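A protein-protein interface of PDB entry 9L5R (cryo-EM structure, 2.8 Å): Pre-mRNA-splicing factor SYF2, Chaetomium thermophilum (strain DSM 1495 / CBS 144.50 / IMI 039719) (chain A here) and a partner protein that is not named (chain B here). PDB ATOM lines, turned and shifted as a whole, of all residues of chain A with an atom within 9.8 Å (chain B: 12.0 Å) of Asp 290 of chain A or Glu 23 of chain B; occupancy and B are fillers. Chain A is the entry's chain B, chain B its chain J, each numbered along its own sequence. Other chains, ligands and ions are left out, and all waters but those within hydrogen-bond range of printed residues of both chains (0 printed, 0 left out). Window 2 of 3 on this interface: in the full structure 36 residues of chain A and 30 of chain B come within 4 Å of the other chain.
NH2 of Arg 27 of chain B is in hydrogen-bond range of O of Gly 289 of chain A (2.9 Å).
The backbone carbonyl oxygen (O) of Thr 292 of chain A is in hydrogen-bond range of the side-chain amide nitrogen (ND2) of Asn 302 of chain A. The side-chain amino group of Lys 299 of chain A lies within hydrogen-bond range of the side-chain hydroxyl of Tyr 293 of chain A, at 3.2 Å. The side-chain carboxylate of Glu 287 of chain A is in hydrogen-bond range of the side-chain hydroxyl of Tyr 293 of chain A, 2.5 Å away. The side-chain carboxylate (OE1) of Glu 287 of chain A is in salt-bridge range of the side-chain amino group (NZ) of Lys 299 of chain A.
Among the printed residues, merely in contact across the chains: Glu 287 of chain A with Arg 27 of chain B, Asp 290 of chain A with Glu 23 of chain B, Val 291 of chain A with Glu 23 of chain B, Val 291 of chain A with Leu 26 of chain B, Val 291 of chain A with Arg 27 of chain B, Val 291 of chain A with Val 30 of chain B, Thr 292 of chain A with Leu 26 of chain B, Tyr 293 of chain A with Val 30 of chain B and Ile 294 of chain A with Val 30 of chain B.
Of chain B, only Arg 27 comes within 4 Å of Gly 289 of chain A. Of chain B, only Glu 23 comes within 4 Å of Asp 290 of chain A. Of chain B, only Leu 26 (3.9 Å) comes within 4 Å of Thr 292 of chain A. Of the printed residues of chain B, Tyr 293 of chain A touches Val 30. No residue of chain A comes within 4 Å of Ala 22 of chain B. Printed residues of chain A within 4 Å of Leu 26 of chain B: Val 291 and Thr 292. The nearest residue of chain B that does not touch Asp 290 of chain A is Arg 27 of chain B (4.5 Å). The nearest printed residue of chain B that does not touch Tyr 293 of chain A is Leu 26 of chain B (4.1 Å).
Hydrophobic or aromatic side chains of chain A that line the printed part of chain B: Val 291. Of the 15 printed residues of chain B, 4 touch a printed residue of chain A. Hydrophobic or aromatic side chains of chain B that line the printed part of chain A: Leu 26 and Val 30. Among the printed residues, no Asp or Glu carboxylate lies within 4 Å of a Lys or Arg side-chain nitrogen of the other chain.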
ATOM      1  N   GLU A 286      35.179  11.303 -15.814  1.00  0.00           N
ATOM      2  CA  GLU A 286      33.730  11.230 -15.983  1.00  0.00           C
ATOM      3  C   GLU A 286      33.063  10.790 -14.683  1.00  0.00           C
ATOM      4  O   GLU A 286      33.618   9.994 -13.922  1.00  0.00           O
ATOM      5  CB  GLU A 286      33.365  10.268 -17.112  1.00  0.00           C
ATOM      6  CG  GLU A 286      33.626  10.826 -18.502  1.00  0.00           C
ATOM      7  CD  GLU A 286      33.216   9.870 -19.606  1.00  0.00           C
ATOM      8  OE1 GLU A 286      32.969   8.682 -19.311  1.00  0.00           O
ATOM      9  OE2 GLU A 286      33.136  10.312 -20.770  1.00  0.00           O
ATOM     10  N   GLU A 287      31.868  11.320 -14.419  1.00  0.00           N
ATOM     11  CA  GLU A 287      31.156  11.054 -13.173  1.00  0.00           C
ATOM     12  C   GLU A 287      29.713  10.689 -13.482  1.00  0.00           C
ATOM     13  O   GLU A 287      28.954  11.520 -13.991  1.00  0.00           O
ATOM     14  CB  GLU A 287      31.217  12.263 -12.233  1.00  0.00           C
ATOM     15  CG  GLU A 287      30.248  12.228 -11.051  1.00  0.00           C
ATOM     16  CD  GLU A 287      30.341  10.955 -10.230  1.00  0.00           C
ATOM     17  OE1 GLU A 287      31.468  10.531  -9.905  1.00  0.00           O
ATOM     18  OE2 GLU A 287      29.288  10.378  -9.907  1.00  0.00           O
ATOM     19  N   HIS A 288      29.334   9.461 -13.156  1.00  0.00           N
ATOM     20  CA  HIS A 288      27.984   8.954 -13.369  1.00  0.00           C
ATOM     21  C   HIS A 288      27.305   8.809 -12.013  1.00  0.00           C
ATOM     22  O   HIS A 288      27.632   7.905 -11.239  1.00  0.00           O
ATOM     23  CB  HIS A 288      28.009   7.619 -14.104  1.00  0.00           C
ATOM     24  CG  HIS A 288      28.395   7.724 -15.545  1.00  0.00           C
ATOM     25  ND1 HIS A 288      28.521   6.620 -16.360  1.00  0.00           N
ATOM     26  CD2 HIS A 288      28.683   8.798 -16.317  1.00  0.00           C
ATOM     27  CE1 HIS A 288      28.869   7.011 -17.573  1.00  0.00           C
ATOM     28  NE2 HIS A 288      28.975   8.327 -17.574  1.00  0.00           N
ATOM     29  N   GLY A 289      26.352   9.687 -11.730  1.00  0.00           N
ATOM     30  CA  GLY A 289      25.571   9.553 -10.521  1.00  0.00           C
ATOM     31  C   GLY A 289      25.991  10.472  -9.395  1.00  0.00           C
ATOM     32  O   GLY A 289      26.389  11.617  -9.625  1.00  0.00           O
ATOM     33  N   ASP A 290      25.913   9.968  -8.170  1.00  0.00           N
ATOM     34  CA  ASP A 290      26.089  10.807  -6.996  1.00  0.00           C
ATOM     35  C   ASP A 290      27.557  11.007  -6.666  1.00  0.00           C
ATOM     36  O   ASP A 290      28.363  10.077  -6.741  1.00  0.00           O
ATOM     37  CB  ASP A 290      25.373  10.192  -5.801  1.00  0.00           C
ATOM     38  CG  ASP A 290      23.883  10.401  -5.852  1.00  0.00           C
ATOM     39  OD1 ASP A 290      23.454  11.487  -6.285  1.00  0.00           O
ATOM     40  OD2 ASP A 290      23.139   9.481  -5.459  1.00  0.00           O
ATOM     41  N   VAL A 291      27.899  12.231  -6.291  1.00  0.00           N
ATOM     42  CA  VAL A 291      29.217  12.514  -5.744  1.00  0.00           C
ATOM     43  C   VAL A 291      29.228  12.052  -4.294  1.00  0.00           C
ATOM     44  O   VAL A 291      28.411  12.496  -3.486  1.00  0.00           O
ATOM     45  CB  VAL A 291      29.557  14.004  -5.865  1.00  0.00           C
ATOM     46  CG1 VAL A 291      30.692  14.374  -4.945  1.00  0.00           C
ATOM     47  CG2 VAL A 291      29.931  14.327  -7.282  1.00  0.00           C
ATOM     48  N   THR A 292      30.135  11.132  -3.972  1.00  0.00           N
ATOM     49  CA  THR A 292      30.293  10.608  -2.621  1.00  0.00           C
ATOM     50  C   THR A 292      31.649  10.959  -2.034  1.00  0.00           C
ATOM     51  O   THR A 292      31.985  10.481  -0.951  1.00  0.00           O
ATOM     52  CB  THR A 292      30.112   9.088  -2.610  1.00  0.00           C
ATOM     53  OG1 THR A 292      30.896   8.508  -3.652  1.00  0.00           O
ATOM     54  CG2 THR A 292      28.672   8.718  -2.830  1.00  0.00           C
ATOM     55  N   TYR A 293      32.426  11.784  -2.719  1.00  0.00           N
ATOM     56  CA  TYR A 293      33.831  12.014  -2.446  1.00  0.00           C
ATOM     57  C   TYR A 293      34.059  13.511  -2.340  1.00  0.00           C
ATOM     58  O   TYR A 293      33.152  14.309  -2.564  1.00  0.00           O
ATOM     59  CB  TYR A 293      34.700  11.406  -3.551  1.00  0.00           C
ATOM     60  CG  TYR A 293      34.152  11.681  -4.933  1.00  0.00           C
ATOM     61  CD1 TYR A 293      34.482  12.845  -5.611  1.00  0.00           C
ATOM     62  CD2 TYR A 293      33.290  10.786  -5.552  1.00  0.00           C
ATOM     63  CE1 TYR A 293      33.972  13.103  -6.849  1.00  0.00           C
ATOM     64  CE2 TYR A 293      32.776  11.042  -6.787  1.00  0.00           C
ATOM     65  CZ  TYR A 293      33.118  12.197  -7.431  1.00  0.00           C
ATOM     66  OH  TYR A 293      32.607  12.445  -8.674  1.00  0.00           O
ATOM     67  N   ILE A 294      35.275  13.907  -1.983  1.00  0.00           N
ATOM     68  CA  ILE A 294      35.582  15.331  -1.886  1.00  0.00           C
ATOM     69  C   ILE A 294      36.867  15.671  -2.619  1.00  0.00           C
ATOM     70  O   ILE A 294      37.183  16.847  -2.796  1.00  0.00           O
ATOM     71  CB  ILE A 294      35.668  15.796  -0.425  1.00  0.00           C
ATOM     72  CG1 ILE A 294      36.628  14.900   0.330  1.00  0.00           C
ATOM     73  CG2 ILE A 294      34.290  15.852   0.224  1.00  0.00           C
ATOM     74  CD1 ILE A 294      36.814  15.312   1.656  1.00  0.00           C
ATOM     75  N   LYS A 299      37.788   9.835  -4.490  1.00  0.00           N
ATOM     76  CA  LYS A 299      37.003   9.221  -5.554  1.00  0.00           C
ATOM     77  C   LYS A 299      37.556   7.852  -5.918  1.00  0.00           C
ATOM     78  O   LYS A 299      36.805   6.881  -6.070  1.00  0.00           O
ATOM     79  CB  LYS A 299      36.995  10.144  -6.766  1.00  0.00           C
ATOM     80  CG  LYS A 299      36.119   9.687  -7.902  1.00  0.00           C
ATOM     81  CD  LYS A 299      35.978  10.784  -8.920  1.00  0.00           C
ATOM     82  CE  LYS A 299      35.336  10.294 -10.182  1.00  0.00           C
ATOM     83  NZ  LYS A 299      33.954   9.842  -9.985  1.00  0.00           N
ATOM     84  N   ASN A 302      36.826   5.440  -3.041  1.00  0.00           N
ATOM     85  CA  ASN A 302      35.427   5.039  -3.009  1.00  0.00           C
ATOM     86  C   ASN A 302      35.097   4.074  -4.132  1.00  0.00           C
ATOM     87  O   ASN A 302      34.266   3.180  -3.952  1.00  0.00           O
ATOM     88  CB  ASN A 302      34.527   6.265  -3.086  1.00  0.00           C
ATOM     89  CG  ASN A 302      34.368   6.955  -1.758  1.00  0.00           C
ATOM     90  OD1 ASN A 302      34.937   6.536  -0.758  1.00  0.00           O
ATOM     91  ND2 ASN A 302      33.603   8.028  -1.742  1.00  0.00           N
ATOM     92  N   ALA A 303      35.737   4.231  -5.294  1.00  0.00           N
ATOM     93  CA  ALA A 303      35.570   3.271  -6.377  1.00  0.00           C
ATOM     94  C   ALA A 303      36.147   1.913  -6.011  1.00  0.00           C
ATOM     95  O   ALA A 303      35.542   0.878  -6.307  1.00  0.00           O
ATOM     96  CB  ALA A 303      36.220   3.799  -7.649  1.00  0.00           C
ATOM     97  N   ARG A 317      22.410  -0.508   1.158  1.00  0.00           N
ATOM     98  CA  ARG A 317      22.311   0.479   0.085  1.00  0.00           C
ATOM     99  C   ARG A 317      20.869   0.678  -0.362  1.00  0.00           C
ATOM    100  O   ARG A 317      20.453   1.808  -0.641  1.00  0.00           O
ATOM    101  CB  ARG A 317      23.180   0.057  -1.093  1.00  0.00           C
ATOM    102  CG  ARG A 317      24.602   0.504  -0.980  1.00  0.00           C
ATOM    103  CD  ARG A 317      25.366   0.221  -2.243  1.00  0.00           C
ATOM    104  NE  ARG A 317      25.634  -1.202  -2.391  1.00  0.00           N
ATOM    105  CZ  ARG A 317      25.332  -1.908  -3.467  1.00  0.00           C
ATOM    106  NH1 ARG A 317      24.776  -1.350  -4.525  1.00  0.00           N
ATOM    107  NH2 ARG A 317      25.591  -3.209  -3.481  1.00  0.00           N
ATOM    108  N   PHE A 320      19.285   2.863   2.260  1.00  0.00           N
ATOM    109  CA  PHE A 320      19.616   4.271   2.075  1.00  0.00           C
ATOM    110  C   PHE A 320      18.956   4.871   0.842  1.00  0.00           C
ATOM    111  O   PHE A 320      18.728   6.081   0.809  1.00  0.00           O
ATOM    112  CB  PHE A 320      21.124   4.459   2.005  1.00  0.00           C
ATOM    113  CG  PHE A 320      21.760   4.620   3.344  1.00  0.00           C
ATOM    114  CD1 PHE A 320      21.271   5.549   4.243  1.00  0.00           C
ATOM    115  CD2 PHE A 320      22.817   3.824   3.723  1.00  0.00           C
ATOM    116  CE1 PHE A 320      21.838   5.693   5.483  1.00  0.00           C
ATOM    117  CE2 PHE A 320      23.373   3.956   4.960  1.00  0.00           C
ATOM    118  CZ  PHE A 320      22.890   4.904   5.839  1.00  0.00           C
ATOM    119  N   GLU A 321      18.647   4.060  -0.168  1.00  0.00           N
ATOM    120  CA  GLU A 321      17.902   4.571  -1.314  1.00  0.00           C
ATOM    121  C   GLU A 321      16.453   4.855  -0.942  1.00  0.00           C
ATOM    122  O   GLU A 321      15.977   5.988  -1.072  1.00  0.00           O
ATOM    123  CB  GLU A 321      17.964   3.580  -2.476  1.00  0.00           C
ATOM    124  CG  GLU A 321      19.261   3.602  -3.237  1.00  0.00           C
ATOM    125  CD  GLU A 321      19.562   2.274  -3.892  1.00  0.00           C
ATOM    126  OE1 GLU A 321      18.637   1.443  -3.986  1.00  0.00           O
ATOM    127  OE2 GLU A 321      20.720   2.055  -4.310  1.00  0.00           O
ATOM    128  N   ILE B  18      12.438  21.603  -4.087  1.00  0.00           N
ATOM    129  CA  ILE B  18      13.704  20.886  -4.125  1.00  0.00           C
ATOM    130  C   ILE B  18      14.211  20.764  -2.697  1.00  0.00           C
ATOM    131  O   ILE B  18      14.376  21.773  -2.003  1.00  0.00           O
ATOM    132  CB  ILE B  18      14.729  21.605  -5.013  1.00  0.00           C
ATOM    133  CG1 ILE B  18      14.385  21.421  -6.487  1.00  0.00           C
ATOM    134  CG2 ILE B  18      16.121  21.099  -4.744  1.00  0.00           C
ATOM    135  CD1 ILE B  18      15.116  22.376  -7.386  1.00  0.00           C
ATOM    136  N   GLN B  19      14.448  19.535  -2.254  1.00  0.00           N
ATOM    137  CA  GLN B  19      14.984  19.266  -0.928  1.00  0.00           C
ATOM    138  C   GLN B  19      16.448  18.875  -1.051  1.00  0.00           C
ATOM    139  O   GLN B  19      16.781  17.965  -1.813  1.00  0.00           O
ATOM    140  CB  GLN B  19      14.195  18.157  -0.235  1.00  0.00           C
ATOM    141  CG  GLN B  19      12.726  18.452  -0.080  1.00  0.00           C
ATOM    142  CD  GLN B  19      12.470  19.632   0.822  1.00  0.00           C
ATOM    143  OE1 GLN B  19      12.753  19.589   2.012  1.00  0.00           O
ATOM    144  NE2 GLN B  19      11.932  20.697   0.257  1.00  0.00           N
ATOM    145  N   ILE B  20      17.311  19.557  -0.287  1.00  0.00           N
ATOM    146  CA  ILE B  20      18.749  19.285  -0.311  1.00  0.00           C
ATOM    147  C   ILE B  20      19.025  17.846   0.131  1.00  0.00           C
ATOM    148  O   ILE B  20      18.210  17.201   0.799  1.00  0.00           O
ATOM    149  CB  ILE B  20      19.489  20.297   0.582  1.00  0.00           C
ATOM    150  CG1 ILE B  20      20.981  20.386   0.256  1.00  0.00           C
ATOM    151  CG2 ILE B  20      19.323  19.948   2.044  1.00  0.00           C
ATOM    152  CD1 ILE B  20      21.289  21.079  -1.014  1.00  0.00           C
ATOM    153  N   SER B  21      20.168  17.323  -0.299  1.00  0.00           N
ATOM    154  CA  SER B  21      20.619  16.011   0.123  1.00  0.00           C
ATOM    155  C   SER B  21      22.114  16.056   0.395  1.00  0.00           C
ATOM    156  O   SER B  21      22.820  16.989  -0.006  1.00  0.00           O
ATOM    157  CB  SER B  21      20.293  14.936  -0.915  1.00  0.00           C
ATOM    158  OG  SER B  21      21.043  15.126  -2.093  1.00  0.00           O
ATOM    159  N   ALA B  22      22.582  15.019   1.093  1.00  0.00           N
ATOM    160  CA  ALA B  22      23.984  14.936   1.481  1.00  0.00           C
ATOM    161  C   ALA B  22      24.891  14.827   0.267  1.00  0.00           C
ATOM    162  O   ALA B  22      25.986  15.396   0.245  1.00  0.00           O
ATOM    163  CB  ALA B  22      24.184  13.748   2.416  1.00  0.00           C
ATOM    164  N   GLU B  23      24.446  14.110  -0.761  1.00  0.00           N
ATOM    165  CA  GLU B  23      25.225  13.994  -1.986  1.00  0.00           C
ATOM    166  C   GLU B  23      25.287  15.312  -2.743  1.00  0.00           C
ATOM    167  O   GLU B  23      26.311  15.620  -3.358  1.00  0.00           O
ATOM    168  CB  GLU B  23      24.639  12.893  -2.855  1.00  0.00           C
ATOM    169  CG  GLU B  23      24.970  11.499  -2.364  1.00  0.00           C
ATOM    170  CD  GLU B  23      24.053  11.017  -1.254  1.00  0.00           C
ATOM    171  OE1 GLU B  23      23.229  11.808  -0.751  1.00  0.00           O
ATOM    172  OE2 GLU B  23      24.153   9.829  -0.881  1.00  0.00           O
ATOM    173  N   GLN B  24      24.212  16.102  -2.700  1.00  0.00           N
ATOM    174  CA  GLN B  24      24.247  17.440  -3.277  1.00  0.00           C
ATOM    175  C   GLN B  24      25.234  18.326  -2.538  1.00  0.00           C
ATOM    176  O   GLN B  24      25.966  19.107  -3.161  1.00  0.00           O
ATOM    177  CB  GLN B  24      22.849  18.057  -3.250  1.00  0.00           C
ATOM    178  CG  GLN B  24      22.737  19.404  -3.951  1.00  0.00           C
ATOM    179  CD  GLN B  24      23.123  19.340  -5.411  1.00  0.00           C
ATOM    180  OE1 GLN B  24      22.827  18.372  -6.099  1.00  0.00           O
ATOM    181  NE2 GLN B  24      23.792  20.374  -5.889  1.00  0.00           N
ATOM    182  N   LEU B  25      25.272  18.212  -1.206  1.00  0.00           N
ATOM    183  CA  LEU B  25      26.264  18.938  -0.415  1.00  0.00           C
ATOM    184  C   LEU B  25      27.685  18.542  -0.790  1.00  0.00           C
ATOM    185  O   LEU B  25      28.563  19.401  -0.919  1.00  0.00           O
ATOM    186  CB  LEU B  25      26.036  18.677   1.065  1.00  0.00           C
ATOM    187  CG  LEU B  25      24.872  19.384   1.729  1.00  0.00           C
ATOM    188  CD1 LEU B  25      24.635  18.768   3.081  1.00  0.00           C
ATOM    189  CD2 LEU B  25      25.183  20.852   1.850  1.00  0.00           C
ATOM    190  N   LEU B  26      27.931  17.242  -0.957  1.00  0.00           N
ATOM    191  CA  LEU B  26      29.258  16.777  -1.347  1.00  0.00           C
ATOM    192  C   LEU B  26      29.643  17.280  -2.730  1.00  0.00           C
ATOM    193  O   LEU B  26      30.794  17.669  -2.954  1.00  0.00           O
ATOM    194  CB  LEU B  26      29.316  15.255  -1.306  1.00  0.00           C
ATOM    195  CG  LEU B  26      29.164  14.681   0.093  1.00  0.00           C
ATOM    196  CD1 LEU B  26      29.145  13.183   0.049  1.00  0.00           C
ATOM    197  CD2 LEU B  26      30.276  15.186   0.975  1.00  0.00           C
ATOM    198  N   ARG B  27      28.694  17.269  -3.670  1.00  0.00           N
ATOM    199  CA  ARG B  27      28.970  17.775  -5.008  1.00  0.00           C
ATOM    200  C   ARG B  27      29.310  19.255  -4.976  1.00  0.00           C
ATOM    201  O   ARG B  27      30.238  19.701  -5.660  1.00  0.00           O
ATOM    202  CB  ARG B  27      27.777  17.526  -5.926  1.00  0.00           C
ATOM    203  CG  ARG B  27      27.975  18.062  -7.329  1.00  0.00           C
ATOM    204  CD  ARG B  27      26.839  17.696  -8.245  1.00  0.00           C
ATOM    205  NE  ARG B  27      26.773  16.267  -8.511  1.00  0.00           N
ATOM    206  CZ  ARG B  27      27.446  15.650  -9.473  1.00  0.00           C
ATOM    207  NH1 ARG B  27      28.291  16.303 -10.252  1.00  0.00           N
ATOM    208  NH2 ARG B  27      27.272  14.346  -9.652  1.00  0.00           N
ATOM    209  N   GLU B  28      28.590  20.026  -4.165  1.00  0.00           N
ATOM    210  CA  GLU B  28      28.890  21.446  -4.048  1.00  0.00           C
ATOM    211  C   GLU B  28      30.241  21.688  -3.380  1.00  0.00           C
ATOM    212  O   GLU B  28      30.956  22.623  -3.750  1.00  0.00           O
ATOM    213  CB  GLU B  28      27.770  22.146  -3.293  1.00  0.00           C
ATOM    214  CG  GLU B  28      26.516  22.308  -4.119  1.00  0.00           C
ATOM    215  CD  GLU B  28      25.272  22.427  -3.273  1.00  0.00           C
ATOM    216  OE1 GLU B  28      25.399  22.475  -2.035  1.00  0.00           O
ATOM    217  OE2 GLU B  28      24.164  22.475  -3.842  1.00  0.00           O
ATOM    218  N   ALA B  29      30.615  20.854  -2.405  1.00  0.00           N
ATOM    219  CA  ALA B  29      31.930  20.984  -1.780  1.00  0.00           C
ATOM    220  C   ALA B  29      33.053  20.681  -2.768  1.00  0.00           C
ATOM    221  O   ALA B  29      34.074  21.381  -2.790  1.00  0.00           O
ATOM    222  CB  ALA B  29      32.027  20.070  -0.563  1.00  0.00           C
ATOM    223  N   VAL B  30      32.876  19.647  -3.593  1.00  0.00           N
ATOM    224  CA  VAL B  30      33.822  19.359  -4.670  1.00  0.00           C
ATOM    225  C   VAL B  30      33.912  20.533  -5.636  1.00  0.00           C
ATOM    226  O   VAL B  30      35.004  20.906  -6.082  1.00  0.00           O
ATOM    227  CB  VAL B  30      33.420  18.062  -5.399  1.00  0.00           C
ATOM    228  CG1 VAL B  30      34.267  17.836  -6.628  1.00  0.00           C
ATOM    229  CG2 VAL B  30      33.562  16.896  -4.489  1.00  0.00           C
ATOM    230  N   ASP B  31      32.767  21.132  -5.977  1.00  0.00           N
ATOM    231  CA  ASP B  31      32.763  22.261  -6.905  1.00  0.00           C
ATOM    232  C   ASP B  31      33.503  23.460  -6.332  1.00  0.00           C
ATOM    233  O   ASP B  31      34.253  24.136  -7.045  1.00  0.00           O
ATOM    234  CB  ASP B  31      31.329  22.651  -7.255  1.00  0.00           C
ATOM    235  CG  ASP B  31      30.633  21.612  -8.100  1.00  0.00           C
ATOM    236  OD1 ASP B  31      31.330  20.765  -8.701  1.00  0.00           O
ATOM    237  OD2 ASP B  31      29.383  21.645  -8.160  1.00  0.00           O
ATOM    238  N   ARG B  32      33.308  23.737  -5.046  1.00  0.00           N
ATOM    239  CA  ARG B  32      34.000  24.835  -4.382  1.00  0.00           C
ATOM    240  C   ARG B  32      35.446  24.510  -4.039  1.00  0.00           C
ATOM    241  O   ARG B  32      36.175  25.407  -3.605  1.00  0.00           O
ATOM    242  CB  ARG B  32      33.247  25.232  -3.110  1.00  0.00           C
ATOM    243  CG  ARG B  32      31.831  25.704  -3.371  1.00  0.00           C
ATOM    244  CD  ARG B  32      31.271  26.519  -2.223  1.00  0.00           C
ATOM    245  NE  ARG B  32      29.903  26.940  -2.503  1.00  0.00           N
ATOM    246  CZ  ARG B  32      29.063  27.418  -1.595  1.00  0.00           C
ATOM    247  NH1 ARG B  32      29.413  27.545  -0.326  1.00  0.00           N
ATOM    248  NH2 ARG B  32      27.838  27.771  -1.971  1.00  0.00           N
